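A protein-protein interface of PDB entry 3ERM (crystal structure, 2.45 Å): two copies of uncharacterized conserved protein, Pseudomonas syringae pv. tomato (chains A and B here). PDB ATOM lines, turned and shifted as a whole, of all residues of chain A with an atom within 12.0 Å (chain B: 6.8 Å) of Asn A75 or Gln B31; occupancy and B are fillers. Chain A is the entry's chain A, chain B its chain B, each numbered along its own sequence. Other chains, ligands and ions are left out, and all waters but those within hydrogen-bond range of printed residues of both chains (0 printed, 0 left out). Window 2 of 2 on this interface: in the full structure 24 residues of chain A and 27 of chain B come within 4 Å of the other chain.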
ATOM      1  N   ARG A  66      28.681  -3.729  -8.265  1.00  0.00           N
ATOM      2  CA  ARG A  66      28.013  -2.907  -7.257  1.00  0.00           C
ATOM      3  C   ARG A  66      26.525  -2.712  -7.520  1.00  0.00           C
ATOM      4  O   ARG A  66      25.750  -2.627  -6.551  1.00  0.00           O
ATOM      5  CB  ARG A  66      28.726  -1.568  -6.972  1.00  0.00           C
ATOM      6  CG  ARG A  66      28.731  -0.597  -8.075  1.00  0.00           C
ATOM      7  CD  ARG A  66      29.559   0.635  -7.713  1.00  0.00           C
ATOM      8  NE  ARG A  66      29.017   1.407  -6.577  1.00  0.00           N
ATOM      9  CZ  ARG A  66      29.611   2.473  -6.025  1.00  0.00           C
ATOM     10  NH1 ARG A  66      30.768   2.937  -6.492  1.00  0.00           N
ATOM     11  NH2 ARG A  66      29.041   3.087  -5.000  1.00  0.00           N
ATOM     12  N   ALA A  67      26.122  -2.667  -8.790  1.00  0.00           N
ATOM     13  CA  ALA A  67      24.710  -2.477  -9.091  1.00  0.00           C
ATOM     14  C   ALA A  67      23.872  -3.707  -8.740  1.00  0.00           C
ATOM     15  O   ALA A  67      22.726  -3.586  -8.319  1.00  0.00           O
ATOM     16  CB  ALA A  67      24.478  -2.027 -10.565  1.00  0.00           C
ATOM     17  N   VAL A  68      24.439  -4.893  -8.906  1.00  0.00           N
ATOM     18  CA  VAL A  68      23.702  -6.108  -8.550  1.00  0.00           C
ATOM     19  C   VAL A  68      23.647  -6.275  -7.039  1.00  0.00           C
ATOM     20  O   VAL A  68      22.627  -6.751  -6.498  1.00  0.00           O
ATOM     21  CB  VAL A  68      24.249  -7.341  -9.232  1.00  0.00           C
ATOM     22  CG1 VAL A  68      23.582  -8.568  -8.682  1.00  0.00           C
ATOM     23  CG2 VAL A  68      24.009  -7.241 -10.740  1.00  0.00           C
ATOM     24  N   PHE A  69      24.721  -5.869  -6.354  1.00  0.00           N
ATOM     25  CA  PHE A  69      24.729  -5.904  -4.886  1.00  0.00           C
ATOM     26  C   PHE A  69      23.808  -4.836  -4.285  1.00  0.00           C
ATOM     27  O   PHE A  69      23.045  -5.135  -3.362  1.00  0.00           O
ATOM     28  CB  PHE A  69      26.153  -5.880  -4.329  1.00  0.00           C
ATOM     29  CG  PHE A  69      26.878  -7.229  -4.466  1.00  0.00           C
ATOM     30  CD1 PHE A  69      27.582  -7.547  -5.620  1.00  0.00           C
ATOM     31  CD2 PHE A  69      26.830  -8.174  -3.451  1.00  0.00           C
ATOM     32  CE1 PHE A  69      28.218  -8.784  -5.755  1.00  0.00           C
ATOM     33  CE2 PHE A  69      27.483  -9.425  -3.571  1.00  0.00           C
ATOM     34  CZ  PHE A  69      28.178  -9.723  -4.718  1.00  0.00           C
ATOM     35  N   ALA A  70      23.824  -3.612  -4.829  1.00  0.00           N
ATOM     36  CA  ALA A  70      22.904  -2.563  -4.388  1.00  0.00           C
ATOM     37  C   ALA A  70      21.451  -3.034  -4.470  1.00  0.00           C
ATOM     38  O   ALA A  70      20.653  -2.801  -3.541  1.00  0.00           O
ATOM     39  CB  ALA A  70      23.093  -1.313  -5.205  1.00  0.00           C
ATOM     40  N   ALA A  71      21.106  -3.722  -5.556  1.00  0.00           N
ATOM     41  CA  ALA A  71      19.734  -4.241  -5.712  1.00  0.00           C
ATOM     42  C   ALA A  71      19.479  -5.352  -4.685  1.00  0.00           C
ATOM     43  O   ALA A  71      18.433  -5.392  -4.047  1.00  0.00           O
ATOM     44  CB  ALA A  71      19.496  -4.747  -7.137  1.00  0.00           C
ATOM     45  N   ALA A  72      20.460  -6.238  -4.515  1.00  0.00           N
ATOM     46  CA  ALA A  72      20.348  -7.314  -3.523  1.00  0.00           C
ATOM     47  C   ALA A  72      20.038  -6.771  -2.121  1.00  0.00           C
ATOM     48  O   ALA A  72      19.067  -7.186  -1.504  1.00  0.00           O
ATOM     49  CB  ALA A  72      21.621  -8.191  -3.499  1.00  0.00           C
ATOM     50  N   PHE A  73      20.876  -5.843  -1.663  1.00  0.00           N
ATOM     51  CA  PHE A  73      20.772  -5.228  -0.348  1.00  0.00           C
ATOM     52  C   PHE A  73      19.573  -4.301  -0.203  1.00  0.00           C
ATOM     53  O   PHE A  73      18.960  -4.288   0.859  1.00  0.00           O
ATOM     54  CB  PHE A  73      22.055  -4.455  -0.008  1.00  0.00           C
ATOM     55  CG  PHE A  73      23.182  -5.324   0.460  1.00  0.00           C
ATOM     56  CD1 PHE A  73      23.456  -5.452   1.802  1.00  0.00           C
ATOM     57  CD2 PHE A  73      23.984  -6.010  -0.442  1.00  0.00           C
ATOM     58  CE1 PHE A  73      24.498  -6.238   2.242  1.00  0.00           C
ATOM     59  CE2 PHE A  73      25.049  -6.803  -0.002  1.00  0.00           C
ATOM     60  CZ  PHE A  73      25.291  -6.919   1.339  1.00  0.00           C
ATOM     61  N   LYS A  74      19.245  -3.523  -1.246  1.00  0.00           N
ATOM     62  CA  LYS A  74      18.069  -2.626  -1.197  1.00  0.00           C
ATOM     63  C   LYS A  74      16.758  -3.362  -0.944  1.00  0.00           C
ATOM     64  O   LYS A  74      15.913  -2.819  -0.250  1.00  0.00           O
ATOM     65  CB  LYS A  74      17.935  -1.683  -2.409  1.00  0.00           C
ATOM     66  CG  LYS A  74      17.134  -0.386  -2.075  1.00  0.00           C
ATOM     67  CD  LYS A  74      16.851   0.600  -3.276  1.00  0.00           C
ATOM     68  CE  LYS A  74      15.556   1.462  -3.053  1.00  0.00           C
ATOM     69  NZ  LYS A  74      15.414   2.689  -3.919  1.00  0.00           N
ATOM     70  N   ASN A  75      16.583  -4.584  -1.468  1.00  0.00           N
ATOM     71  CA  ASN A  75      15.284  -5.318  -1.311  1.00  0.00           C
ATOM     72  C   ASN A  75      15.253  -6.866  -1.431  1.00  0.00           C
ATOM     73  O   ASN A  75      15.138  -7.597  -0.410  1.00  0.00           O
ATOM     74  CB  ASN A  75      14.214  -4.719  -2.244  1.00  0.00           C
ATOM     75  CG  ASN A  75      14.811  -4.145  -3.536  1.00  0.00           C
ATOM     76  OD1 ASN A  75      14.438  -3.042  -3.963  1.00  0.00           O
ATOM     77  ND2 ASN A  75      15.756  -4.882  -4.150  1.00  0.00           N
ATOM     78  N   ASN A  76      15.291  -7.333  -2.688  1.00  0.00           N
ATOM     79  CA  ASN A  76      15.349  -8.759  -3.021  1.00  0.00           C
ATOM     80  C   ASN A  76      16.787  -9.299  -3.048  1.00  0.00           C
ATOM     81  O   ASN A  76      17.583  -9.012  -3.960  1.00  0.00           O
ATOM     82  CB  ASN A  76      14.603  -9.066  -4.331  1.00  0.00           C
ATOM     83  CG  ASN A  76      15.193  -8.337  -5.544  1.00  0.00           C
ATOM     84  OD1 ASN A  76      14.650  -8.425  -6.641  1.00  0.00           O
ATOM     85  ND2 ASN A  76      16.309  -7.627  -5.351  1.00  0.00           N
ATOM     86  N   ALA A  77      17.105 -10.069  -2.013  1.00  0.00           N
ATOM     87  CA  ALA A  77      18.306 -10.864  -2.006  1.00  0.00           C
ATOM     88  C   ALA A  77      18.477 -11.543  -3.371  1.00  0.00           C
ATOM     89  O   ALA A  77      19.596 -11.691  -3.858  1.00  0.00           O
ATOM     90  CB  ALA A  77      18.241 -11.899  -0.882  1.00  0.00           C
ATOM     91  N   THR A  78      17.365 -11.909  -4.002  1.00  0.00           N
ATOM     92  CA  THR A  78      17.392 -12.741  -5.197  1.00  0.00           C
ATOM     93  C   THR A  78      18.067 -12.124  -6.411  1.00  0.00           C
ATOM     94  O   THR A  78      18.358 -12.823  -7.373  1.00  0.00           O
ATOM     95  CB  THR A  78      15.989 -13.168  -5.611  1.00  0.00           C
ATOM     96  OG1 THR A  78      15.190 -11.997  -5.849  1.00  0.00           O
ATOM     97  CG2 THR A  78      15.354 -14.030  -4.529  1.00  0.00           C
ATOM     98  N   ALA A  79      18.321 -10.826  -6.392  1.00  0.00           N
ATOM     99  CA  ALA A  79      18.953 -10.230  -7.545  1.00  0.00           C
ATOM    100  C   ALA A  79      20.402 -10.738  -7.751  1.00  0.00           C
ATOM    101  O   ALA A  79      20.968 -10.621  -8.842  1.00  0.00           O
ATOM    102  CB  ALA A  79      18.878  -8.734  -7.470  1.00  0.00           C
ATOM    103  N   LEU A  80      20.981 -11.335  -6.709  1.00  0.00           N
ATOM    104  CA  LEU A  80      22.324 -11.959  -6.764  1.00  0.00           C
ATOM    105  C   LEU A  80      22.368 -13.130  -7.746  1.00  0.00           C
ATOM    106  O   LEU A  80      23.420 -13.461  -8.268  1.00  0.00           O
ATOM    107  CB  LEU A  80      22.754 -12.433  -5.385  1.00  0.00           C
ATOM    108  CG  LEU A  80      22.866 -11.376  -4.298  1.00  0.00           C
ATOM    109  CD1 LEU A  80      22.880 -12.102  -2.983  1.00  0.00           C
ATOM    110  CD2 LEU A  80      24.144 -10.480  -4.468  1.00  0.00           C
ATOM    111  N   SER A  81      21.219 -13.749  -7.972  1.00  0.00           N
ATOM    112  CA  SER A  81      21.018 -14.613  -9.126  1.00  0.00           C
ATOM    113  C   SER A  81      21.464 -14.050 -10.467  1.00  0.00           C
ATOM    114  O   SER A  81      21.766 -14.823 -11.375  1.00  0.00           O
ATOM    115  CB  SER A  81      19.559 -14.998  -9.268  1.00  0.00           C
ATOM    116  OG  SER A  81      19.438 -16.314  -8.802  1.00  0.00           O
ATOM    117  N   GLU A  82      21.474 -12.721 -10.609  1.00  0.00           N
ATOM    118  CA  GLU A  82      21.914 -12.084 -11.869  1.00  0.00           C
ATOM    119  C   GLU A  82      23.443 -12.063 -12.057  1.00  0.00           C
ATOM    120  O   GLU A  82      23.933 -11.713 -13.125  1.00  0.00           O
ATOM    121  CB  GLU A  82      21.326 -10.672 -12.011  1.00  0.00           C
ATOM    122  CG  GLU A  82      19.796 -10.638 -12.054  1.00  0.00           C
ATOM    123  CD  GLU A  82      19.223  -9.228 -12.087  1.00  0.00           C
ATOM    124  OE1 GLU A  82      19.932  -8.294 -12.543  1.00  0.00           O
ATOM    125  OE2 GLU A  82      18.053  -9.071 -11.666  1.00  0.00           O
ATOM    126  N   ALA B  26      10.253 -11.512  13.832  1.00  0.00           N
ATOM    127  CA  ALA B  26      10.811 -12.807  13.340  1.00  0.00           C
ATOM    128  C   ALA B  26      11.062 -12.835  11.817  1.00  0.00           C
ATOM    129  O   ALA B  26      12.098 -13.360  11.369  1.00  0.00           O
ATOM    130  CB  ALA B  26       9.941 -13.983  13.759  1.00  0.00           C
ATOM    131  N   ASP B  27      10.141 -12.258  11.025  1.00  0.00           N
ATOM    132  CA  ASP B  27      10.362 -12.137   9.569  1.00  0.00           C
ATOM    133  C   ASP B  27      11.383 -11.052   9.168  1.00  0.00           C
ATOM    134  O   ASP B  27      12.029 -11.150   8.106  1.00  0.00           O
ATOM    135  CB  ASP B  27       9.060 -12.096   8.747  1.00  0.00           C
ATOM    136  CG  ASP B  27       8.021 -11.139   9.309  1.00  0.00           C
ATOM    137  OD1 ASP B  27       8.321  -9.928   9.455  1.00  0.00           O
ATOM    138  OD2 ASP B  27       6.883 -11.597   9.574  1.00  0.00           O
ATOM    139  N   ALA B  28      11.576 -10.057  10.038  1.00  0.00           N
ATOM    140  CA  ALA B  28      12.743  -9.166   9.922  1.00  0.00           C
ATOM    141  C   ALA B  28      13.970 -10.025   9.733  1.00  0.00           C
ATOM    142  O   ALA B  28      14.707  -9.864   8.753  1.00  0.00           O
ATOM    143  CB  ALA B  28      12.914  -8.333  11.182  1.00  0.00           C
ATOM    144  N   HIS B  29      14.168 -10.952  10.675  1.00  0.00           N
ATOM    145  CA  HIS B  29      15.397 -11.739  10.739  1.00  0.00           C
ATOM    146  C   HIS B  29      15.470 -12.718   9.579  1.00  0.00           C
ATOM    147  O   HIS B  29      16.568 -13.022   9.090  1.00  0.00           O
ATOM    148  CB  HIS B  29      15.515 -12.520  12.065  1.00  0.00           C
ATOM    149  CG  HIS B  29      15.319 -11.692  13.302  1.00  0.00           C
ATOM    150  ND1 HIS B  29      16.149 -10.645  13.644  1.00  0.00           N
ATOM    151  CD2 HIS B  29      14.408 -11.792  14.305  1.00  0.00           C
ATOM    152  CE1 HIS B  29      15.747 -10.130  14.795  1.00  0.00           C
ATOM    153  NE2 HIS B  29      14.707 -10.820  15.224  1.00  0.00           N
ATOM    154  N   ASP B  30      14.302 -13.202   9.154  1.00  0.00           N
ATOM    155  CA  ASP B  30      14.182 -14.190   8.072  1.00  0.00           C
ATOM    156  C   ASP B  30      14.792 -13.613   6.791  1.00  0.00           C
ATOM    157  O   ASP B  30      15.549 -14.297   6.066  1.00  0.00           O
ATOM    158  CB  ASP B  30      12.713 -14.525   7.822  1.00  0.00           C
ATOM    159  CG  ASP B  30      12.108 -15.430   8.880  1.00  0.00           C
ATOM    160  OD1 ASP B  30      10.856 -15.454   8.999  1.00  0.00           O
ATOM    161  OD2 ASP B  30      12.856 -16.150   9.567  1.00  0.00           O
ATOM    162  N   GLN B  31      14.471 -12.338   6.569  1.00  0.00           N
ATOM    163  CA  GLN B  31      14.950 -11.512   5.473  1.00  0.00           C
ATOM    164  C   GLN B  31      16.462 -11.398   5.498  1.00  0.00           C
ATOM    165  O   GLN B  31      17.183 -11.702   4.504  1.00  0.00           O
ATOM    166  CB  GLN B  31      14.332 -10.128   5.673  1.00  0.00           C
ATOM    167  CG  GLN B  31      14.373  -9.224   4.483  1.00  0.00           C
ATOM    168  CD  GLN B  31      13.316  -9.589   3.471  1.00  0.00           C
ATOM    169  OE1 GLN B  31      13.069  -8.850   2.482  1.00  0.00           O
ATOM    170  NE2 GLN B  31      12.664 -10.741   3.702  1.00  0.00           N
ATOM    171  N   MET B  32      16.932 -10.963   6.664  1.00  0.00           N
ATOM    172  CA  MET B  32      18.339 -10.813   6.931  1.00  0.00           C
ATOM    173  C   MET B  32      19.046 -12.162   6.689  1.00  0.00           C
ATOM    174  O   MET B  32      20.089 -12.243   6.002  1.00  0.00           O
ATOM    175  CB  MET B  32      18.461 -10.363   8.379  1.00  0.00           C
ATOM    176  CG  MET B  32      19.812  -9.914   8.837  1.00  0.00           C
ATOM    177  SD  MET B  32      20.848 -11.387   9.532  1.00  0.00           S
ATOM    178  CE  MET B  32      21.805 -11.859   7.958  1.00  0.00           C
ATOM    179  N   LEU B  33      18.461 -13.233   7.211  1.00  0.00           N
ATOM    180  CA  LEU B  33      19.136 -14.553   7.130  1.00  0.00           C
ATOM    181  C   LEU B  33      19.170 -15.082   5.701  1.00  0.00           C
ATOM    182  O   LEU B  33      20.162 -15.639   5.253  1.00  0.00           O
ATOM    183  CB  LEU B  33      18.523 -15.575   8.091  1.00  0.00           C
ATOM    184  CG  LEU B  33      18.780 -15.182   9.547  1.00  0.00           C
ATOM    185  CD1 LEU B  33      17.693 -15.714  10.496  1.00  0.00           C
ATOM    186  CD2 LEU B  33      20.146 -15.584  10.008  1.00  0.00           C
ATOM    187  N   GLU B  34      18.088 -14.850   4.983  1.00  0.00           N
ATOM    188  CA  GLU B  34      17.980 -15.303   3.621  1.00  0.00           C
ATOM    189  C   GLU B  34      19.046 -14.620   2.749  1.00  0.00           C
ATOM    190  O   GLU B  34      19.786 -15.289   2.021  1.00  0.00           O
ATOM    191  CB  GLU B  34      16.582 -14.997   3.154  1.00  0.00           C
ATOM    192  CG  GLU B  34      16.394 -15.149   1.707  1.00  0.00           C
ATOM    193  CD  GLU B  34      14.946 -15.096   1.356  1.00  0.00           C
ATOM    194  OE1 GLU B  34      14.118 -15.531   2.205  1.00  0.00           O
ATOM    195  OE2 GLU B  34      14.630 -14.621   0.234  1.00  0.00           O
ATOM    196  N   LEU B  35      19.158 -13.301   2.866  1.00  0.00           N
ATOM    197  CA  LEU B  35      20.181 -12.559   2.151  1.00  0.00           C
ATOM    198  C   LEU B  35      21.588 -13.072   2.475  1.00  0.00           C
ATOM    199  O   LEU B  35      22.324 -13.457   1.552  1.00  0.00           O
ATOM    200  CB  LEU B  35      20.037 -11.057   2.431  1.00  0.00           C
ATOM    201  CG  LEU B  35      21.248 -10.207   2.060  1.00  0.00           C
ATOM    202  CD1 LEU B  35      21.450 -10.104   0.565  1.00  0.00           C
ATOM    203  CD2 LEU B  35      21.135  -8.822   2.724  1.00  0.00           C
ATOM    204  N   ALA B  36      21.925 -13.126   3.779  1.00  0.00           N
ATOM    205  CA  ALA B  36      23.181 -13.708   4.291  1.00  0.00           C
ATOM    206  C   ALA B  36      23.552 -15.008   3.590  1.00  0.00           C
ATOM    207  O   ALA B  36      24.714 -15.229   3.183  1.00  0.00           O
ATOM    208  CB  ALA B  36      23.084 -13.965   5.788  1.00  0.00           C
ATOM    209  N   ALA B  63      24.747  -8.408   5.814  1.00  0.00           N
ATOM    210  CA  ALA B  63      23.289  -8.550   5.694  1.00  0.00           C
ATOM    211  C   ALA B  63      22.608  -7.899   6.902  1.00  0.00           C
ATOM    212  O   ALA B  63      21.547  -7.298   6.809  1.00  0.00           O
ATOM    213  CB  ALA B  63      22.898 -10.037   5.600  1.00  0.00           C
ATOM    214  N   ARG B  66      22.336  -4.167   6.290  1.00  0.00           N
ATOM    215  CA  ARG B  66      22.032  -4.082   4.867  1.00  0.00           C
ATOM    216  C   ARG B  66      21.762  -2.693   4.353  1.00  0.00           C
ATOM    217  O   ARG B  66      22.205  -2.384   3.250  1.00  0.00           O
ATOM    218  CB  ARG B  66      20.960  -5.084   4.393  1.00  0.00           C
ATOM    219  CG  ARG B  66      19.548  -4.832   4.843  1.00  0.00           C
ATOM    220  CD  ARG B  66      18.606  -5.943   4.341  1.00  0.00           C
ATOM    221  NE  ARG B  66      18.663  -6.160   2.879  1.00  0.00           N
ATOM    222  CZ  ARG B  66      17.754  -6.834   2.151  1.00  0.00           C
ATOM    223  NH1 ARG B  66      16.672  -7.360   2.698  1.00  0.00           N
ATOM    224  NH2 ARG B  66      17.911  -6.990   0.853  1.00  0.00           N
ATOM    225  N   ALA B  70      23.579  -1.127   1.286  1.00  0.00           N
ATOM    226  CA  ALA B  70      22.755  -0.722   0.147  1.00  0.00           C
ATOM    227  C   ALA B  70      23.090   0.680  -0.236  1.00  0.00           C
ATOM    228  O   ALA B  70      23.271   0.968  -1.411  1.00  0.00           O
ATOM    229  CB  ALA B  70      21.245  -0.821   0.444  1.00  0.00           C
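The guanidinium group (NH2) of Arg B66 sits at hydrogen-bond distance from the backbone carbonyl oxygen (O) of Asn A75 (3.1 Å).
O of Phe A73 is in hydrogen-bond range of NE of Arg B66.
The backbone carbonyl oxygen of Ala A72 lies within hydrogen-bond range of the guanidinium group of Arg B66.
The side-chain amide nitrogen (ND2) of Asn A76 lies close to the side-chain amide nitrogen (ND2) of Asn A75, 3.0 Å away.
The side-chain amide nitrogen of Asn A75 lies within hydrogen-bond range of the backbone carbonyl oxygen of Ala A71 (2.7 Å).
Phe A73 touches Ala B70.
Ala B70 touches Lys A74.
O of Asn A75 touches OE1 of Gln B31, 3.8 Å away.
Ala A77 touches Leu B35 (CB to CA, 3.7 Å).
Of chain B, only Gln B31 and Arg B66 come within 4 Å of Asn A75.
Asp B30 touches none of the printed residues of chain A.
No residue of chain A comes within 4 Å of Met B32.
Leu B33 touches none of the printed residues of chain A.
Glu B34 touches none of the printed residues of chain A.
Of the printed residues of chain B, Ala A72 touches Arg B66 (2.6 Å).
Printed residues of chain B within 4 Å of Phe A73: Arg B66 (2.8 Å) and Ala B70 (3.8 Å).
Printed residues of chain B within 4 Å of Ala A77: Leu B35.
Of the printed residues of chain A, Ala B70 touches Phe A73 (3.8 Å) and Lys A74 (3.8 Å).
Of the printed residues of chain B, Lys A74 touches Ala B70 (3.8 Å).
The nearest residue of chain B that does not touch Asn A75 is Ala B70 (6.3 Å).
The nearest residue of chain A that does not touch Gln B31 is Ala A77 (5.5 Å).
The nearest printed residue of chain B that does not touch Lys A74 is Arg B66 (4.2 Å).
Of the 17 printed residues of chain A, 5 touch a printed residue of chain B.
Hydrophobic or aromatic side chains of chain B within 4 Å of the printed part of chain A: Leu B35 and Ala B70.
Among the printed residues, 7 pairs touch across the chains.
Among the printed residues, no Asp or Glu carboxylate lies within 4 Å of a Lys or Arg side-chain nitrogen of the other chain.
Positions printed for both chains: 66 and 70.
Of the 7 pairs that touch across the chains among the printed residues, none has its exchanged pair printed and touching as well.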
